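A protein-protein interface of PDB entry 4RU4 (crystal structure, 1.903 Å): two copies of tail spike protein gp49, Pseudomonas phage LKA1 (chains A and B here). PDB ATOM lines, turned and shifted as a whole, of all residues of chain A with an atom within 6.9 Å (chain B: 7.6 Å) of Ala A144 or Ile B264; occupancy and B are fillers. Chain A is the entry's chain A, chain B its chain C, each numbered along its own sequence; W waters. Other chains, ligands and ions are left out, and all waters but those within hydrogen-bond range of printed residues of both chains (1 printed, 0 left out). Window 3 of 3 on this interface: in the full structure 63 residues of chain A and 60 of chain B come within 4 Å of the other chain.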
ATOM      1  N   LEU A 142      19.465 -31.659   8.970  1.00  0.00           N
ATOM      2  CA  LEU A 142      19.642 -31.195   7.595  1.00  0.00           C
ATOM      3  C   LEU A 142      21.081 -30.750   7.414  1.00  0.00           C
ATOM      4  O   LEU A 142      21.678 -30.214   8.344  1.00  0.00           O
ATOM      5  CB  LEU A 142      18.746 -29.997   7.330  1.00  0.00           C
ATOM      6  CG  LEU A 142      17.228 -30.219   7.383  1.00  0.00           C
ATOM      7  CD1 LEU A 142      16.520 -28.894   7.336  1.00  0.00           C
ATOM      8  CD2 LEU A 142      16.770 -31.113   6.221  1.00  0.00           C
ATOM      9  N   VAL A 143      21.630 -30.978   6.223  1.00  0.00           N
ATOM     10  CA  VAL A 143      22.894 -30.364   5.821  1.00  0.00           C
ATOM     11  C   VAL A 143      22.731 -29.746   4.436  1.00  0.00           C
ATOM     12  O   VAL A 143      21.703 -29.949   3.770  1.00  0.00           O
ATOM     13  CB  VAL A 143      24.062 -31.384   5.784  1.00  0.00           C
ATOM     14  CG1 VAL A 143      24.295 -31.985   7.183  1.00  0.00           C
ATOM     15  CG2 VAL A 143      23.775 -32.499   4.746  1.00  0.00           C
ATOM     16  N   ALA A 144      23.751 -29.001   4.001  1.00  0.00           N
ATOM     17  CA  ALA A 144      23.739 -28.344   2.694  1.00  0.00           C
ATOM     18  C   ALA A 144      23.379 -29.340   1.572  1.00  0.00           C
ATOM     19  O   ALA A 144      23.901 -30.451   1.548  1.00  0.00           O
ATOM     20  CB  ALA A 144      25.121 -27.702   2.432  1.00  0.00           C
ATOM     21  N   GLY A 145      22.465 -28.959   0.677  1.00  0.00           N
ATOM     22  CA  GLY A 145      22.042 -29.835  -0.410  1.00  0.00           C
ATOM     23  C   GLY A 145      20.790 -30.659  -0.113  1.00  0.00           C
ATOM     24  O   GLY A 145      20.146 -31.198  -1.034  1.00  0.00           O
ATOM     25  N   ASP A 146      20.450 -30.782   1.165  1.00  0.00           N
ATOM     26  CA  ASP A 146      19.240 -31.518   1.551  1.00  0.00           C
ATOM     27  C   ASP A 146      17.990 -30.817   1.040  1.00  0.00           C
ATOM     28  O   ASP A 146      17.995 -29.596   0.870  1.00  0.00           O
ATOM     29  CB  ASP A 146      19.125 -31.695   3.057  1.00  0.00           C
ATOM     30  CG  ASP A 146      20.017 -32.802   3.589  1.00  0.00           C
ATOM     31  OD1 ASP A 146      20.607 -33.561   2.783  1.00  0.00           O
ATOM     32  OD2 ASP A 146      20.125 -32.894   4.834  1.00  0.00           O
ATOM     33  N   VAL A 147      16.935 -31.598   0.806  1.00  0.00           N
ATOM     34  CA  VAL A 147      15.647 -31.063   0.352  1.00  0.00           C
ATOM     35  C   VAL A 147      14.518 -31.291   1.347  1.00  0.00           C
ATOM     36  O   VAL A 147      14.344 -32.410   1.880  1.00  0.00           O
ATOM     37  CB  VAL A 147      15.280 -31.648  -1.039  1.00  0.00           C
ATOM     38  CG1 VAL A 147      13.894 -31.164  -1.491  1.00  0.00           C
ATOM     39  CG2 VAL A 147      16.356 -31.230  -2.080  1.00  0.00           C
ATOM     40  N   GLU A 172      15.736 -26.030  -0.749  1.00  0.00           N
ATOM     41  CA  GLU A 172      17.022 -26.716  -0.831  1.00  0.00           C
ATOM     42  C   GLU A 172      17.999 -26.055   0.129  1.00  0.00           C
ATOM     43  O   GLU A 172      18.199 -24.841   0.054  1.00  0.00           O
ATOM     44  CB  GLU A 172      17.538 -26.627  -2.262  1.00  0.00           C
ATOM     45  CG  GLU A 172      18.713 -27.519  -2.564  1.00  0.00           C
ATOM     46  CD  GLU A 172      19.057 -27.486  -4.033  1.00  0.00           C
ATOM     47  OE1 GLU A 172      18.128 -27.309  -4.877  1.00  0.00           O
ATOM     48  OE2 GLU A 172      20.263 -27.615  -4.350  1.00  0.00           O
ATOM     49  N   VAL A 173      18.623 -26.846   1.010  1.00  0.00           N
ATOM     50  CA  VAL A 173      19.394 -26.273   2.111  1.00  0.00           C
ATOM     51  C   VAL A 173      20.699 -25.641   1.619  1.00  0.00           C
ATOM     52  O   VAL A 173      21.466 -26.261   0.860  1.00  0.00           O
ATOM     53  CB  VAL A 173      19.679 -27.327   3.226  1.00  0.00           C
ATOM     54  CG1 VAL A 173      20.656 -26.765   4.247  1.00  0.00           C
ATOM     55  CG2 VAL A 173      18.359 -27.783   3.888  1.00  0.00           C
ATOM     56  N   ARG A 174      20.939 -24.400   2.025  1.00  0.00           N
ATOM     57  CA  ARG A 174      22.221 -23.771   1.710  1.00  0.00           C
ATOM     58  C   ARG A 174      23.254 -23.996   2.810  1.00  0.00           C
ATOM     59  O   ARG A 174      24.376 -24.454   2.546  1.00  0.00           O
ATOM     60  CB  ARG A 174      22.044 -22.277   1.452  1.00  0.00           C
ATOM     61  CG  ARG A 174      23.290 -21.602   0.905  1.00  0.00           C
ATOM     62  CD  ARG A 174      23.011 -20.137   0.643  1.00  0.00           C
ATOM     63  NE  ARG A 174      23.201 -19.293   1.820  1.00  0.00           N
ATOM     64  CZ  ARG A 174      22.306 -18.416   2.286  1.00  0.00           C
ATOM     65  NH1 ARG A 174      21.114 -18.260   1.686  1.00  0.00           N
ATOM     66  NH2 ARG A 174      22.606 -17.678   3.363  1.00  0.00           N
ATOM     67  N   ALA A 175      22.872 -23.666   4.039  1.00  0.00           N
ATOM     68  CA  ALA A 175      23.734 -23.834   5.207  1.00  0.00           C
ATOM     69  C   ALA A 175      22.894 -24.011   6.466  1.00  0.00           C
ATOM     70  O   ALA A 175      21.706 -23.700   6.490  1.00  0.00           O
ATOM     71  CB  ALA A 175      24.665 -22.628   5.359  1.00  0.00           C
ATOM     72  N   VAL A 176      23.521 -24.532   7.515  1.00  0.00           N
ATOM     73  CA  VAL A 176      22.847 -24.753   8.785  1.00  0.00           C
ATOM     74  C   VAL A 176      23.741 -24.207   9.884  1.00  0.00           C
ATOM     75  O   VAL A 176      24.943 -24.491   9.914  1.00  0.00           O
ATOM     76  CB  VAL A 176      22.603 -26.252   9.058  1.00  0.00           C
ATOM     77  CG1 VAL A 176      21.844 -26.442  10.370  1.00  0.00           C
ATOM     78  CG2 VAL A 176      21.857 -26.894   7.897  1.00  0.00           C
ATOM     79  N   ARG A 184      18.530 -22.117  -0.759  1.00  0.00           N
ATOM     80  CA  ARG A 184      19.242 -21.693  -1.962  1.00  0.00           C
ATOM     81  C   ARG A 184      18.438 -20.788  -2.902  1.00  0.00           C
ATOM     82  O   ARG A 184      19.010 -20.143  -3.775  1.00  0.00           O
ATOM     83  CB  ARG A 184      19.797 -22.914  -2.705  1.00  0.00           C
ATOM     84  CG  ARG A 184      20.826 -23.647  -1.872  1.00  0.00           C
ATOM     85  CD  ARG A 184      21.341 -24.900  -2.580  1.00  0.00           C
ATOM     86  NE  ARG A 184      22.606 -25.310  -1.960  1.00  0.00           N
ATOM     87  CZ  ARG A 184      23.269 -26.417  -2.280  1.00  0.00           C
ATOM     88  NH1 ARG A 184      22.780 -27.245  -3.209  1.00  0.00           N
ATOM     89  NH2 ARG A 184      24.417 -26.683  -1.679  1.00  0.00           N
ATOM     90  N   GLY B 216      34.185 -32.787  -1.986  1.00  0.00           N
ATOM     91  CA  GLY B 216      34.640 -32.271  -0.693  1.00  0.00           C
ATOM     92  C   GLY B 216      35.293 -30.891  -0.788  1.00  0.00           C
ATOM     93  O   GLY B 216      34.954 -30.070  -1.674  1.00  0.00           O
ATOM     94  N   THR B 217      36.246 -30.618   0.106  1.00  0.00           N
ATOM     95  CA  THR B 217      36.747 -29.253   0.269  1.00  0.00           C
ATOM     96  C   THR B 217      38.105 -29.019  -0.361  1.00  0.00           C
ATOM     97  O   THR B 217      38.543 -27.875  -0.498  1.00  0.00           O
ATOM     98  CB  THR B 217      36.892 -28.874   1.762  1.00  0.00           C
ATOM     99  OG1 THR B 217      37.706 -29.856   2.414  1.00  0.00           O
ATOM    100  CG2 THR B 217      35.535 -28.820   2.450  1.00  0.00           C
ATOM    101  N   VAL B 238      27.908 -33.571  -9.586  1.00  0.00           N
ATOM    102  CA  VAL B 238      29.156 -33.160  -8.957  1.00  0.00           C
ATOM    103  C   VAL B 238      28.860 -32.276  -7.753  1.00  0.00           C
ATOM    104  O   VAL B 238      28.057 -31.352  -7.850  1.00  0.00           O
ATOM    105  CB  VAL B 238      30.034 -32.360  -9.933  1.00  0.00           C
ATOM    106  CG1 VAL B 238      31.293 -31.796  -9.190  1.00  0.00           C
ATOM    107  CG2 VAL B 238      30.422 -33.208 -11.150  1.00  0.00           C
ATOM    108  N   THR B 239      29.478 -32.562  -6.610  1.00  0.00           N
ATOM    109  CA  THR B 239      29.345 -31.667  -5.483  1.00  0.00           C
ATOM    110  C   THR B 239      30.761 -31.319  -5.080  1.00  0.00           C
ATOM    111  O   THR B 239      31.688 -32.084  -5.352  1.00  0.00           O
ATOM    112  CB  THR B 239      28.547 -32.280  -4.309  1.00  0.00           C
ATOM    113  OG1 THR B 239      29.298 -33.361  -3.741  1.00  0.00           O
ATOM    114  CG2 THR B 239      27.159 -32.785  -4.789  1.00  0.00           C
ATOM    115  N   LEU B 240      30.936 -30.143  -4.496  1.00  0.00           N
ATOM    116  CA  LEU B 240      32.262 -29.652  -4.152  1.00  0.00           C
ATOM    117  C   LEU B 240      32.044 -28.496  -3.185  1.00  0.00           C
ATOM    118  O   LEU B 240      30.936 -27.976  -3.101  1.00  0.00           O
ATOM    119  CB  LEU B 240      32.948 -29.127  -5.420  1.00  0.00           C
ATOM    120  CG  LEU B 240      34.440 -28.780  -5.345  1.00  0.00           C
ATOM    121  CD1 LEU B 240      35.263 -30.046  -5.351  1.00  0.00           C
ATOM    122  CD2 LEU B 240      34.826 -27.844  -6.484  1.00  0.00           C
ATOM    123  N   ALA B 241      33.084 -28.112  -2.445  1.00  0.00           N
ATOM    124  CA  ALA B 241      33.070 -26.900  -1.635  1.00  0.00           C
ATOM    125  C   ALA B 241      34.399 -26.210  -1.873  1.00  0.00           C
ATOM    126  O   ALA B 241      35.214 -26.064  -0.954  1.00  0.00           O
ATOM    127  CB  ALA B 241      32.890 -27.197  -0.134  1.00  0.00           C
ATOM    128  N   ASN B 242      34.616 -25.793  -3.118  1.00  0.00           N
ATOM    129  CA  ASN B 242      35.847 -25.118  -3.503  1.00  0.00           C
ATOM    130  C   ASN B 242      35.608 -24.226  -4.739  1.00  0.00           C
ATOM    131  O   ASN B 242      34.563 -23.569  -4.832  1.00  0.00           O
ATOM    132  CB  ASN B 242      36.955 -26.150  -3.758  1.00  0.00           C
ATOM    133  CG  ASN B 242      38.364 -25.565  -3.596  1.00  0.00           C
ATOM    134  OD1 ASN B 242      38.821 -24.794  -4.438  1.00  0.00           O
ATOM    135  ND2 ASN B 242      39.069 -25.971  -2.534  1.00  0.00           N
ATOM    136  N   ASN B 243      36.531 -24.226  -5.704  1.00  0.00           N
ATOM    137  CA  ASN B 243      36.465 -23.209  -6.767  1.00  0.00           C
ATOM    138  C   ASN B 243      35.470 -23.408  -7.915  1.00  0.00           C
ATOM    139  O   ASN B 243      34.755 -22.468  -8.292  1.00  0.00           O
ATOM    140  CB  ASN B 243      37.857 -22.860  -7.334  1.00  0.00           C
ATOM    141  CG  ASN B 243      37.879 -21.442  -7.958  1.00  0.00           C
ATOM    142  OD1 ASN B 243      37.660 -20.429  -7.268  1.00  0.00           O
ATOM    143  ND2 ASN B 243      38.116 -21.375  -9.245  1.00  0.00           N
ATOM    144  N   ILE B 261      25.040 -29.890 -10.734  1.00  0.00           N
ATOM    145  CA  ILE B 261      26.330 -29.419 -10.257  1.00  0.00           C
ATOM    146  C   ILE B 261      26.042 -28.539  -9.056  1.00  0.00           C
ATOM    147  O   ILE B 261      25.180 -27.681  -9.111  1.00  0.00           O
ATOM    148  CB  ILE B 261      27.084 -28.616 -11.362  1.00  0.00           C
ATOM    149  CG1 ILE B 261      27.114 -29.400 -12.695  1.00  0.00           C
ATOM    150  CG2 ILE B 261      28.468 -28.188 -10.873  1.00  0.00           C
ATOM    151  CD1 ILE B 261      27.985 -30.691 -12.675  1.00  0.00           C
ATOM    152  N   SER B 262      26.738 -28.787  -7.959  1.00  0.00           N
ATOM    153  CA  SER B 262      26.468 -28.065  -6.731  1.00  0.00           C
ATOM    154  C   SER B 262      27.786 -27.724  -6.068  1.00  0.00           C
ATOM    155  O   SER B 262      28.440 -28.595  -5.501  1.00  0.00           O
ATOM    156  CB  SER B 262      25.624 -28.932  -5.784  1.00  0.00           C
ATOM    157  OG  SER B 262      25.403 -28.272  -4.539  1.00  0.00           O
ATOM    158  N   ASN B 263      28.173 -26.458  -6.122  1.00  0.00           N
ATOM    159  CA  ASN B 263      29.396 -26.030  -5.460  1.00  0.00           C
ATOM    160  C   ASN B 263      29.104 -25.082  -4.306  1.00  0.00           C
ATOM    161  O   ASN B 263      28.715 -23.921  -4.502  1.00  0.00           O
ATOM    162  CB  ASN B 263      30.353 -25.384  -6.452  1.00  0.00           C
ATOM    163  CG  ASN B 263      31.648 -24.969  -5.802  1.00  0.00           C
ATOM    164  OD1 ASN B 263      31.949 -25.401  -4.681  1.00  0.00           O
ATOM    165  ND2 ASN B 263      32.420 -24.130  -6.489  1.00  0.00           N
ATOM    166  N   ILE B 264      29.282 -25.596  -3.105  1.00  0.00           N
ATOM    167  CA  ILE B 264      29.097 -24.841  -1.872  1.00  0.00           C
ATOM    168  C   ILE B 264      30.091 -23.687  -1.816  1.00  0.00           C
ATOM    169  O   ILE B 264      29.820 -22.653  -1.205  1.00  0.00           O
ATOM    170  CB  ILE B 264      29.221 -25.784  -0.647  1.00  0.00           C
ATOM    171  CG1 ILE B 264      27.990 -26.705  -0.557  1.00  0.00           C
ATOM    172  CG2 ILE B 264      29.495 -25.014   0.666  1.00  0.00           C
ATOM    173  CD1 ILE B 264      28.194 -27.878   0.400  1.00  0.00           C
ATOM    174  N   GLY B 265      31.226 -23.859  -2.488  1.00  0.00           N
ATOM    175  CA  GLY B 265      32.254 -22.831  -2.564  1.00  0.00           C
ATOM    176  C   GLY B 265      33.204 -22.903  -1.371  1.00  0.00           C
ATOM    177  O   GLY B 265      32.874 -23.504  -0.332  1.00  0.00           O
ATOM    178  N   ASP B 266      34.371 -22.278  -1.498  1.00  0.00           N
ATOM    179  CA  ASP B 266      35.248 -22.097  -0.338  1.00  0.00           C
ATOM    180  C   ASP B 266      35.535 -20.631  -0.137  1.00  0.00           C
ATOM    181  O   ASP B 266      36.578 -20.291   0.381  1.00  0.00           O
ATOM    182  CB  ASP B 266      36.582 -22.828  -0.523  1.00  0.00           C
ATOM    183  CG  ASP B 266      37.382 -22.311  -1.720  1.00  0.00           C
ATOM    184  OD1 ASP B 266      36.817 -21.584  -2.575  1.00  0.00           O
ATOM    185  OD2 ASP B 266      38.586 -22.644  -1.814  1.00  0.00           O
ATOM    186  N   GLY B 267      34.656 -19.759  -0.614  1.00  0.00           N
ATOM    187  CA  GLY B 267      34.851 -18.333  -0.417  1.00  0.00           C
ATOM    188  C   GLY B 267      35.723 -17.657  -1.464  1.00  0.00           C
ATOM    189  O   GLY B 267      36.132 -16.516  -1.293  1.00  0.00           O
ATOM    190  N   ASP B 270      34.170 -19.482  -6.675  1.00  0.00           N
ATOM    191  CA  ASP B 270      33.004 -20.313  -6.342  1.00  0.00           C
ATOM    192  C   ASP B 270      31.965 -20.434  -7.481  1.00  0.00           C
ATOM    193  O   ASP B 270      30.830 -19.937  -7.383  1.00  0.00           O
ATOM    194  CB  ASP B 270      32.359 -19.770  -5.071  1.00  0.00           C
ATOM    195  CG  ASP B 270      33.260 -19.910  -3.844  1.00  0.00           C
ATOM    196  OD1 ASP B 270      34.426 -20.366  -3.972  1.00  0.00           O
ATOM    197  OD2 ASP B 270      32.788 -19.573  -2.743  1.00  0.00           O
ATOM    198  N   TYR B 271      32.387 -21.088  -8.550  1.00  0.00           N
ATOM    199  CA  TYR B 271      31.591 -21.318  -9.755  1.00  0.00           C
ATOM    200  C   TYR B 271      30.942 -22.687  -9.742  1.00  0.00           C
ATOM    201  O   TYR B 271      31.510 -23.626  -9.219  1.00  0.00           O
ATOM    202  CB  TYR B 271      32.538 -21.360 -10.951  1.00  0.00           C
ATOM    203  CG  TYR B 271      33.298 -20.090 -11.229  1.00  0.00           C
ATOM    204  CD1 TYR B 271      32.655 -18.867 -11.334  1.00  0.00           C
ATOM    205  CD2 TYR B 271      34.669 -20.122 -11.418  1.00  0.00           C
ATOM    206  CE1 TYR B 271      33.384 -17.689 -11.622  1.00  0.00           C
ATOM    207  CE2 TYR B 271      35.391 -18.959 -11.681  1.00  0.00           C
ATOM    208  CZ  TYR B 271      34.745 -17.751 -11.795  1.00  0.00           C
ATOM    209  OH  TYR B 271      35.495 -16.610 -12.059  1.00  0.00           O
ATOM    210  N   TYR B 289      23.740 -25.219  -8.669  1.00  0.00           N
ATOM    211  CA  TYR B 289      23.921 -24.270  -7.558  1.00  0.00           C
ATOM    212  C   TYR B 289      25.420 -23.954  -7.398  1.00  0.00           C
ATOM    213  O   TYR B 289      26.260 -24.842  -7.527  1.00  0.00           O
ATOM    214  CB  TYR B 289      23.375 -24.826  -6.215  1.00  0.00           C
ATOM    215  CG  TYR B 289      23.805 -23.936  -5.073  1.00  0.00           C
ATOM    216  CD1 TYR B 289      23.105 -22.765  -4.782  1.00  0.00           C
ATOM    217  CD2 TYR B 289      24.966 -24.205  -4.355  1.00  0.00           C
ATOM    218  CE1 TYR B 289      23.511 -21.912  -3.762  1.00  0.00           C
ATOM    219  CE2 TYR B 289      25.410 -23.321  -3.357  1.00  0.00           C
ATOM    220  CZ  TYR B 289      24.670 -22.191  -3.063  1.00  0.00           C
ATOM    221  OH  TYR B 289      25.085 -21.339  -2.066  1.00  0.00           O
ATOM    222  N   ALA B 290      25.756 -22.701  -7.099  1.00  0.00           N
ATOM    223  CA  ALA B 290      27.097 -22.380  -6.603  1.00  0.00           C
ATOM    224  C   ALA B 290      27.024 -21.120  -5.790  1.00  0.00           C
ATOM    225  O   ALA B 290      26.159 -20.289  -6.034  1.00  0.00           O
ATOM    226  CB  ALA B 290      28.101 -22.212  -7.753  1.00  0.00           C
ATOM    227  N   ARG B 291      27.958 -20.936  -4.861  1.00  0.00           N
ATOM    228  CA  ARG B 291      27.819 -19.816  -3.944  1.00  0.00           C
ATOM    229  C   ARG B 291      27.738 -18.460  -4.688  1.00  0.00           C
ATOM    230  O   ARG B 291      26.876 -17.647  -4.387  1.00  0.00           O
ATOM    231  CB  ARG B 291      28.946 -19.777  -2.891  1.00  0.00           C
ATOM    232  CG  ARG B 291      28.680 -18.726  -1.806  1.00  0.00           C
ATOM    233  CD  ARG B 291      29.851 -18.596  -0.826  1.00  0.00           C
ATOM    234  NE  ARG B 291      31.033 -18.050  -1.503  1.00  0.00           N
ATOM    235  CZ  ARG B 291      31.350 -16.755  -1.586  1.00  0.00           C
ATOM    236  NH1 ARG B 291      30.570 -15.819  -1.035  1.00  0.00           N
ATOM    237  NH2 ARG B 291      32.456 -16.390  -2.227  1.00  0.00           N
ATOM    238  N   ARG B 292      28.638 -18.228  -5.644  1.00  0.00           N
ATOM    239  CA  ARG B 292      28.673 -16.972  -6.376  1.00  0.00           C
ATOM    240  C   ARG B 292      27.976 -17.059  -7.742  1.00  0.00           C
ATOM    241  O   ARG B 292      26.968 -16.391  -7.944  1.00  0.00           O
ATOM    242  CB  ARG B 292      30.100 -16.424  -6.502  1.00  0.00           C
ATOM    243  CG  ARG B 292      30.600 -15.746  -5.191  1.00  0.00           C
ATOM    244  CD  ARG B 292      32.011 -15.192  -5.361  1.00  0.00           C
ATOM    245  NE  ARG B 292      32.068 -14.214  -6.450  1.00  0.00           N
ATOM    246  CZ  ARG B 292      31.717 -12.942  -6.293  1.00  0.00           C
ATOM    247  NH1 ARG B 292      31.282 -12.511  -5.094  1.00  0.00           N
ATOM    248  NH2 ARG B 292      31.799 -12.094  -7.324  1.00  0.00           N
ATOM    249  N   ASP B 321      24.029 -18.242  -3.753  1.00  0.00           N
ATOM    250  CA  ASP B 321      23.865 -17.764  -2.383  1.00  0.00           C
ATOM    251  C   ASP B 321      23.532 -16.272  -2.477  1.00  0.00           C
ATOM    252  O   ASP B 321      24.388 -15.448  -2.825  1.00  0.00           O
ATOM    253  CB  ASP B 321      25.174 -17.987  -1.615  1.00  0.00           C
ATOM    254  CG  ASP B 321      25.165 -17.398  -0.206  1.00  0.00           C
ATOM    255  OD1 ASP B 321      24.166 -16.805   0.276  1.00  0.00           O
ATOM    256  OD2 ASP B 321      26.208 -17.573   0.453  1.00  0.00           O
HETATM  257  O   HOH W   1      25.342 -18.260   3.134  1.00  0.00           O
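CD1 of Ile B264 touches CB of Ala A144 (3.7 Å).
Arg A174 touches Tyr B289 (CG to OH, 3.5 Å).
Arg A184 touches Ile B264.
Tyr B289 touches Arg A184.
Water W1 bridges NE of Arg A174 (2.7 Å) and OD2 of Asp B321 (2.9 Å).
Of the 12 printed residues of chain A, 3 touch a printed residue of chain B.
Among the printed residues, Asp or Glu carboxylates within 4 Å of a Lys or Arg side-chain nitrogen of the other chain: Arg A174 with Asp B321 (3.1 Å).
Printed residues of chain B within 4 Å of Arg A174: Tyr B289 and Asp B321.
Of the printed residues of chain B, Arg A184 touches Ser B262, Ile B264 and Tyr B289.
Gly B216 touches none of the printed residues of chain A.
Thr B239 touches none of the printed residues of chain A.
Of chain A, only Ala A144 (3.7 Å) and Arg A184 (3.7 Å) come within 4 Å of Ile B264.
Of the printed residues of chain A, Tyr B289 touches Arg A174 and Arg A184.
Of the printed residues of chain A, Asp B321 touches Arg A174 (3.1 Å).
No position is printed for both chains.
The guanidinium group (NE) of Arg A174 lies within salt-bridge range of the side-chain carboxylate (OD1) of Asp B321, at 3.1 Å.
NH1 of Arg A184 sits at hydrogen-bond distance from OG of Ser B262, 3.1 Å away.
O of Val A173 lies within hydrogen-bond range of NE of Arg A184, at 3.2 Å.
The backbone carbonyl oxygen (O) of Val B238 lies within hydrogen-bond range of the backbone NH (N) of Ser B262, 2.9 Å away.
N of Leu B240 lies within hydrogen-bond range of O of Ser B262.
The backbone NH of Tyr B289 sits at hydrogen-bond distance from the backbone carbonyl oxygen of Ile B261 (2.9 Å).
The backbone NH (N) of Asn B263 is in hydrogen-bond range of the backbone carbonyl oxygen (O) of Tyr B289 (2.9 Å).
The backbone carbonyl oxygen of Arg B291 sits at hydrogen-bond distance from the backbone NH of Asp B321.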
